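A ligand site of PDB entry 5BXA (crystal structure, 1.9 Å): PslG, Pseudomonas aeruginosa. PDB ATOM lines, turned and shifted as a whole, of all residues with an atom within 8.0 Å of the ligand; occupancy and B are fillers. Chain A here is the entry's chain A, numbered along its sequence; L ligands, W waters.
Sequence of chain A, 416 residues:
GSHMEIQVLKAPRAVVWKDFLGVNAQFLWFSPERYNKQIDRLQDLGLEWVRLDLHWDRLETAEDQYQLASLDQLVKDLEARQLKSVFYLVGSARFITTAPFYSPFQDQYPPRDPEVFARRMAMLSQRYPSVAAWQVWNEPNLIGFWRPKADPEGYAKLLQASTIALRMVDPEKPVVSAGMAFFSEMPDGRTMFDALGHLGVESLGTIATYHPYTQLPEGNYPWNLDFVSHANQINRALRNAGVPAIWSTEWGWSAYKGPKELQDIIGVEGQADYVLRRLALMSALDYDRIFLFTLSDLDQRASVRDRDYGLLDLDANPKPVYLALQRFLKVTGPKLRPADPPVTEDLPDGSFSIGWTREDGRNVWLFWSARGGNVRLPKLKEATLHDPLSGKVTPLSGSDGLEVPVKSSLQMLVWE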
ATOM      1  N   GLN A  26     -11.674  -7.158  -5.357  1.00  0.00           N
ATOM      2  CA  GLN A  26     -12.808  -7.913  -4.882  1.00  0.00           C
ATOM      3  C   GLN A  26     -13.754  -6.992  -4.119  1.00  0.00           C
ATOM      4  O   GLN A  26     -14.140  -7.297  -3.004  1.00  0.00           O
ATOM      5  CB  GLN A  26     -12.345  -9.066  -3.977  1.00  0.00           C
ATOM      6  CG  GLN A  26     -12.021 -10.363  -4.702  1.00  0.00           C
ATOM      7  CD  GLN A  26     -10.729 -10.266  -5.500  1.00  0.00           C
ATOM      8  OE1 GLN A  26      -9.795  -9.566  -5.122  1.00  0.00           O
ATOM      9  NE2 GLN A  26     -10.667 -10.979  -6.625  1.00  0.00           N
ATOM     10  N   PHE A  27     -14.106  -5.862  -4.735  1.00  0.00           N
ATOM     11  CA  PHE A  27     -14.781  -4.796  -4.009  1.00  0.00           C
ATOM     12  C   PHE A  27     -16.112  -5.210  -3.367  1.00  0.00           C
ATOM     13  O   PHE A  27     -16.472  -4.710  -2.307  1.00  0.00           O
ATOM     14  CB  PHE A  27     -15.001  -3.595  -4.942  1.00  0.00           C
ATOM     15  CG  PHE A  27     -13.726  -2.895  -5.339  1.00  0.00           C
ATOM     16  CD1 PHE A  27     -12.678  -2.758  -4.440  1.00  0.00           C
ATOM     17  CD2 PHE A  27     -13.579  -2.367  -6.609  1.00  0.00           C
ATOM     18  CE1 PHE A  27     -11.506  -2.110  -4.794  1.00  0.00           C
ATOM     19  CE2 PHE A  27     -12.414  -1.703  -6.987  1.00  0.00           C
ATOM     20  CZ  PHE A  27     -11.375  -1.569  -6.083  1.00  0.00           C
ATOM     21  N   LEU A  28     -16.840  -6.125  -4.004  1.00  0.00           N
ATOM     22  CA  LEU A  28     -18.131  -6.570  -3.452  1.00  0.00           C
ATOM     23  C   LEU A  28     -17.983  -7.293  -2.109  1.00  0.00           C
ATOM     24  O   LEU A  28     -18.979  -7.549  -1.424  1.00  0.00           O
ATOM     25  CB  LEU A  28     -18.854  -7.476  -4.452  1.00  0.00           C
ATOM     26  CG  LEU A  28     -19.321  -6.791  -5.733  1.00  0.00           C
ATOM     27  CD1 LEU A  28     -19.898  -7.803  -6.711  1.00  0.00           C
ATOM     28  CD2 LEU A  28     -20.360  -5.723  -5.401  1.00  0.00           C
ATOM     29  N   TRP A  29     -16.749  -7.625  -1.746  1.00  0.00           N
ATOM     30  CA  TRP A  29     -16.486  -8.250  -0.444  1.00  0.00           C
ATOM     31  C   TRP A  29     -16.421  -7.237   0.673  1.00  0.00           C
ATOM     32  O   TRP A  29     -16.322  -7.608   1.844  1.00  0.00           O
ATOM     33  CB  TRP A  29     -15.146  -8.999  -0.446  1.00  0.00           C
ATOM     34  CG  TRP A  29     -15.073 -10.237  -1.256  1.00  0.00           C
ATOM     35  CD1 TRP A  29     -15.437 -10.399  -2.565  1.00  0.00           C
ATOM     36  CD2 TRP A  29     -14.514 -11.496  -0.836  1.00  0.00           C
ATOM     37  NE1 TRP A  29     -15.160 -11.684  -2.972  1.00  0.00           N
ATOM     38  CE2 TRP A  29     -14.593 -12.371  -1.933  1.00  0.00           C
ATOM     39  CE3 TRP A  29     -13.964 -11.949   0.366  1.00  0.00           C
ATOM     40  CZ2 TRP A  29     -14.150 -13.692  -1.853  1.00  0.00           C
ATOM     41  CZ3 TRP A  29     -13.520 -13.249   0.439  1.00  0.00           C
ATOM     42  CH2 TRP A  29     -13.618 -14.111  -0.665  1.00  0.00           C
ATOM     43  N   PHE A  30     -16.439  -5.958   0.323  1.00  0.00           N
ATOM     44  CA  PHE A  30     -16.174  -4.909   1.287  1.00  0.00           C
ATOM     45  C   PHE A  30     -17.254  -3.830   1.300  1.00  0.00           C
ATOM     46  O   PHE A  30     -17.991  -3.642   0.332  1.00  0.00           O
ATOM     47  CB  PHE A  30     -14.830  -4.247   0.973  1.00  0.00           C
ATOM     48  CG  PHE A  30     -13.656  -5.196   1.023  1.00  0.00           C
ATOM     49  CD1 PHE A  30     -12.981  -5.423   2.218  1.00  0.00           C
ATOM     50  CD2 PHE A  30     -13.200  -5.817  -0.135  1.00  0.00           C
ATOM     51  CE1 PHE A  30     -11.871  -6.267   2.264  1.00  0.00           C
ATOM     52  CE2 PHE A  30     -12.087  -6.670  -0.088  1.00  0.00           C
ATOM     53  CZ  PHE A  30     -11.433  -6.893   1.116  1.00  0.00           C
ATOM     54  N   LEU A  52     -12.892  -7.023 -11.933  1.00  0.00           N
ATOM     55  CA  LEU A  52     -13.771  -7.512 -10.881  1.00  0.00           C
ATOM     56  C   LEU A  52     -14.508  -8.771 -11.297  1.00  0.00           C
ATOM     57  O   LEU A  52     -14.891  -8.918 -12.464  1.00  0.00           O
ATOM     58  CB  LEU A  52     -14.781  -6.424 -10.488  1.00  0.00           C
ATOM     59  CG  LEU A  52     -14.099  -5.327  -9.681  1.00  0.00           C
ATOM     60  CD1 LEU A  52     -14.533  -3.959 -10.162  1.00  0.00           C
ATOM     61  CD2 LEU A  52     -14.398  -5.501  -8.200  1.00  0.00           C
ATOM     62  N   ASP A  53     -14.723  -9.674 -10.347  1.00  0.00           N
ATOM     63  CA  ASP A  53     -15.393 -10.930 -10.623  1.00  0.00           C
ATOM     64  C   ASP A  53     -16.877 -10.841 -10.268  1.00  0.00           C
ATOM     65  O   ASP A  53     -17.230 -10.348  -9.198  1.00  0.00           O
ATOM     66  CB  ASP A  53     -14.746 -12.069  -9.844  1.00  0.00           C
ATOM     67  CG  ASP A  53     -14.673 -11.798  -8.351  1.00  0.00           C
ATOM     68  OD1 ASP A  53     -14.176 -10.722  -7.945  1.00  0.00           O
ATOM     69  OD2 ASP A  53     -15.114 -12.670  -7.580  1.00  0.00           O
ATOM     70  N   LEU A  54     -17.723 -11.315 -11.177  1.00  0.00           N
ATOM     71  CA  LEU A  54     -19.142 -11.467 -10.924  1.00  0.00           C
ATOM     72  C   LEU A  54     -19.511 -12.938 -10.997  1.00  0.00           C
ATOM     73  O   LEU A  54     -19.176 -13.613 -11.953  1.00  0.00           O
ATOM     74  CB  LEU A  54     -19.973 -10.685 -11.926  1.00  0.00           C
ATOM     75  CG  LEU A  54     -19.730  -9.174 -11.933  1.00  0.00           C
ATOM     76  CD1 LEU A  54     -20.588  -8.500 -13.014  1.00  0.00           C
ATOM     77  CD2 LEU A  54     -20.047  -8.609 -10.557  1.00  0.00           C
ATOM     78  N   HIS A  55     -20.203 -13.444  -9.994  1.00  0.00           N
ATOM     79  CA  HIS A  55     -20.626 -14.823 -10.037  1.00  0.00           C
ATOM     80  C   HIS A  55     -22.112 -14.867 -10.249  1.00  0.00           C
ATOM     81  O   HIS A  55     -22.870 -14.344  -9.446  1.00  0.00           O
ATOM     82  CB  HIS A  55     -20.198 -15.547  -8.781  1.00  0.00           C
ATOM     83  CG  HIS A  55     -18.713 -15.630  -8.630  1.00  0.00           C
ATOM     84  ND1 HIS A  55     -18.001 -16.777  -8.931  1.00  0.00           N
ATOM     85  CD2 HIS A  55     -17.801 -14.704  -8.269  1.00  0.00           C
ATOM     86  CE1 HIS A  55     -16.717 -16.550  -8.740  1.00  0.00           C
ATOM     87  NE2 HIS A  55     -16.567 -15.306  -8.327  1.00  0.00           N
ATOM     88  N   ASP A  57     -24.443 -17.031  -9.969  1.00  0.00           N
ATOM     89  CA  ASP A  57     -25.330 -17.629  -8.982  1.00  0.00           C
ATOM     90  C   ASP A  57     -25.467 -16.751  -7.724  1.00  0.00           C
ATOM     91  O   ASP A  57     -26.353 -16.981  -6.916  1.00  0.00           O
ATOM     92  CB  ASP A  57     -24.857 -19.054  -8.605  1.00  0.00           C
ATOM     93  CG  ASP A  57     -23.629 -19.057  -7.700  1.00  0.00           C
ATOM     94  OD1 ASP A  57     -22.770 -18.161  -7.824  1.00  0.00           O
ATOM     95  OD2 ASP A  57     -23.516 -19.991  -6.873  1.00  0.00           O
ATOM     96  N   ARG A  58     -24.622 -15.745  -7.589  1.00  0.00           N
ATOM     97  CA  ARG A  58     -24.788 -14.780  -6.531  1.00  0.00           C
ATOM     98  C   ARG A  58     -25.589 -13.562  -6.938  1.00  0.00           C
ATOM     99  O   ARG A  58     -26.112 -12.867  -6.118  1.00  0.00           O
ATOM    100  CB  ARG A  58     -23.441 -14.341  -6.023  1.00  0.00           C
ATOM    101  CG  ARG A  58     -22.940 -15.167  -4.895  1.00  0.00           C
ATOM    102  CD  ARG A  58     -21.676 -15.840  -5.268  1.00  0.00           C
ATOM    103  NE  ARG A  58     -20.480 -15.127  -4.858  1.00  0.00           N
ATOM    104  CZ  ARG A  58     -19.254 -15.617  -5.005  1.00  0.00           C
ATOM    105  NH1 ARG A  58     -18.202 -14.921  -4.648  1.00  0.00           N
ATOM    106  NH2 ARG A  58     -19.096 -16.818  -5.498  1.00  0.00           N
ATOM    107  N   LEU A  59     -25.639 -13.287  -8.216  1.00  0.00           N
ATOM    108  CA  LEU A  59     -26.376 -12.126  -8.728  1.00  0.00           C
ATOM    109  C   LEU A  59     -27.818 -12.467  -9.084  1.00  0.00           C
ATOM    110  O   LEU A  59     -28.708 -11.612  -9.007  1.00  0.00           O
ATOM    111  CB  LEU A  59     -25.674 -11.543  -9.945  1.00  0.00           C
ATOM    112  CG  LEU A  59     -24.301 -10.917  -9.660  1.00  0.00           C
ATOM    113  CD1 LEU A  59     -23.695 -10.433 -10.950  1.00  0.00           C
ATOM    114  CD2 LEU A  59     -24.413  -9.787  -8.635  1.00  0.00           C
ATOM    115  N   GLN A  67     -29.955  -9.875  -7.223  1.00  0.00           N
ATOM    116  CA  GLN A  67     -29.392  -9.223  -6.041  1.00  0.00           C
ATOM    117  C   GLN A  67     -28.373  -8.222  -6.541  1.00  0.00           C
ATOM    118  O   GLN A  67     -27.180  -8.539  -6.603  1.00  0.00           O
ATOM    119  CB  GLN A  67     -28.726 -10.234  -5.106  1.00  0.00           C
ATOM    120  CG  GLN A  67     -29.563 -11.459  -4.805  1.00  0.00           C
ATOM    121  CD  GLN A  67     -30.556 -11.218  -3.694  1.00  0.00           C
ATOM    122  OE1 GLN A  67     -30.440 -10.244  -2.946  1.00  0.00           O
ATOM    123  NE2 GLN A  67     -31.541 -12.103  -3.560  1.00  0.00           N
ATOM    124  N   SER A  70     -25.822  -4.019  -4.299  1.00  0.00           N
ATOM    125  CA  SER A  70     -24.387  -3.779  -4.022  1.00  0.00           C
ATOM    126  C   SER A  70     -23.603  -3.464  -5.284  1.00  0.00           C
ATOM    127  O   SER A  70     -22.740  -2.578  -5.279  1.00  0.00           O
ATOM    128  CB  SER A  70     -23.752  -4.992  -3.341  1.00  0.00           C
ATOM    129  OG  SER A  70     -24.280  -5.167  -2.039  1.00  0.00           O
ATOM    130  N   LEU A 298      -8.003 -10.776   1.715  1.00  0.00           N
ATOM    131  CA  LEU A 298      -9.427 -11.101   1.899  1.00  0.00           C
ATOM    132  C   LEU A 298      -9.642 -11.795   3.221  1.00  0.00           C
ATOM    133  O   LEU A 298      -8.688 -12.284   3.826  1.00  0.00           O
ATOM    134  CB  LEU A 298      -9.926 -12.003   0.756  1.00  0.00           C
ATOM    135  CG  LEU A 298      -9.698 -11.469  -0.658  1.00  0.00           C
ATOM    136  CD1 LEU A 298      -9.972 -12.551  -1.676  1.00  0.00           C
ATOM    137  CD2 LEU A 298     -10.570 -10.242  -0.918  1.00  0.00           C
ATOM    138  N   ASP A 299     -10.895 -11.857   3.665  1.00  0.00           N
ATOM    139  CA  ASP A 299     -11.196 -12.469   4.954  1.00  0.00           C
ATOM    140  C   ASP A 299     -11.432 -13.985   4.845  1.00  0.00           C
ATOM    141  O   ASP A 299     -11.134 -14.589   3.814  1.00  0.00           O
ATOM    142  CB  ASP A 299     -12.405 -11.784   5.620  1.00  0.00           C
ATOM    143  CG  ASP A 299     -13.713 -11.973   4.838  1.00  0.00           C
ATOM    144  OD1 ASP A 299     -13.808 -12.871   3.975  1.00  0.00           O
ATOM    145  OD2 ASP A 299     -14.670 -11.215   5.128  1.00  0.00           O
ATOM    146  N   ARG A 301     -13.752 -15.832   4.185  1.00  0.00           N
ATOM    147  CA  ARG A 301     -14.551 -16.382   3.093  1.00  0.00           C
ATOM    148  C   ARG A 301     -13.645 -16.942   1.990  1.00  0.00           C
ATOM    149  O   ARG A 301     -14.061 -17.792   1.206  1.00  0.00           O
ATOM    150  CB  ARG A 301     -15.487 -15.324   2.514  1.00  0.00           C
ATOM    151  CG  ARG A 301     -16.726 -15.052   3.351  1.00  0.00           C
ATOM    152  CD  ARG A 301     -17.440 -13.818   2.851  1.00  0.00           C
ATOM    153  NE  ARG A 301     -16.638 -12.622   3.061  1.00  0.00           N
ATOM    154  CZ  ARG A 301     -16.980 -11.405   2.631  1.00  0.00           C
ATOM    155  NH1 ARG A 301     -18.105 -11.236   1.946  1.00  0.00           N
ATOM    156  NH2 ARG A 301     -16.192 -10.368   2.888  1.00  0.00           N
ATOM    157  N   ALA A 302     -12.405 -16.467   1.948  1.00  0.00           N
ATOM    158  CA  ALA A 302     -11.432 -16.971   0.990  1.00  0.00           C
ATOM    159  C   ALA A 302     -10.639 -18.119   1.586  1.00  0.00           C
ATOM    160  O   ALA A 302     -10.468 -18.190   2.798  1.00  0.00           O
ATOM    161  CB  ALA A 302     -10.491 -15.860   0.550  1.00  0.00           C
HETATM  162  C1  LIG L   1     -19.296 -11.944  -3.849  1.00  0.00           C
HETATM  163  C2  LIG L   1     -20.461 -11.214  -3.127  1.00  0.00           C
HETATM  164  C3  LIG L   1     -20.283 -11.265  -1.601  1.00  0.00           C
HETATM  165  C4  LIG L   1     -19.732 -12.623  -1.179  1.00  0.00           C
HETATM  166  C5  LIG L   1     -18.293 -12.750  -1.674  1.00  0.00           C
HETATM  167  C6  LIG L   1     -17.748 -14.176  -1.608  1.00  0.00           C
HETATM  168  O1  LIG L   1     -18.981 -11.119  -4.972  1.00  0.00           O
HETATM  169  O2  LIG L   1     -21.692 -11.864  -3.402  1.00  0.00           O
HETATM  170  O3  LIG L   1     -21.496 -10.977  -0.921  1.00  0.00           O
HETATM  171  O4  LIG L   1     -19.741 -12.725   0.243  1.00  0.00           O
HETATM  172  O5  LIG L   1     -18.146 -12.238  -3.054  1.00  0.00           O
HETATM  173  O6  LIG L   1     -18.816 -15.088  -1.864  1.00  0.00           O
HETATM  174  O   HOH W   1     -22.538 -10.812  -5.789  1.00  0.00           O
HETATM  175  O   HOH W   2     -20.837 -11.786  -7.703  1.00  0.00           O
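Residues that only touch the ligand: Leu 28 (3.7 Å).
Hydrophobic or aromatic side chains within 4 Å of the ligand: Leu 28 and Trp 29.
The backbone carbonyl oxygen (O) of Trp 29 is in hydrogen-bond range of the guanidinium group (NH2) of Arg 301 (3.0 Å).
OD2 of Asp 299 lies within salt-bridge range of NH2 of Arg 301 (2.8 Å).
NH1 of Arg 301 lies within hydrogen-bond range of O4 of the ligand, at 2.8 Å.
The indole nitrogen (NE1) of Trp 29 lies within hydrogen-bond range of an oxygen (O5) of the ligand (3.0 Å).
The guanidinium group (NH1) of Arg 58 lies within hydrogen-bond range of an oxygen (O6) of the ligand (2.9 Å).
Water W2 bridges N of His 55 and O1 of the ligand.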
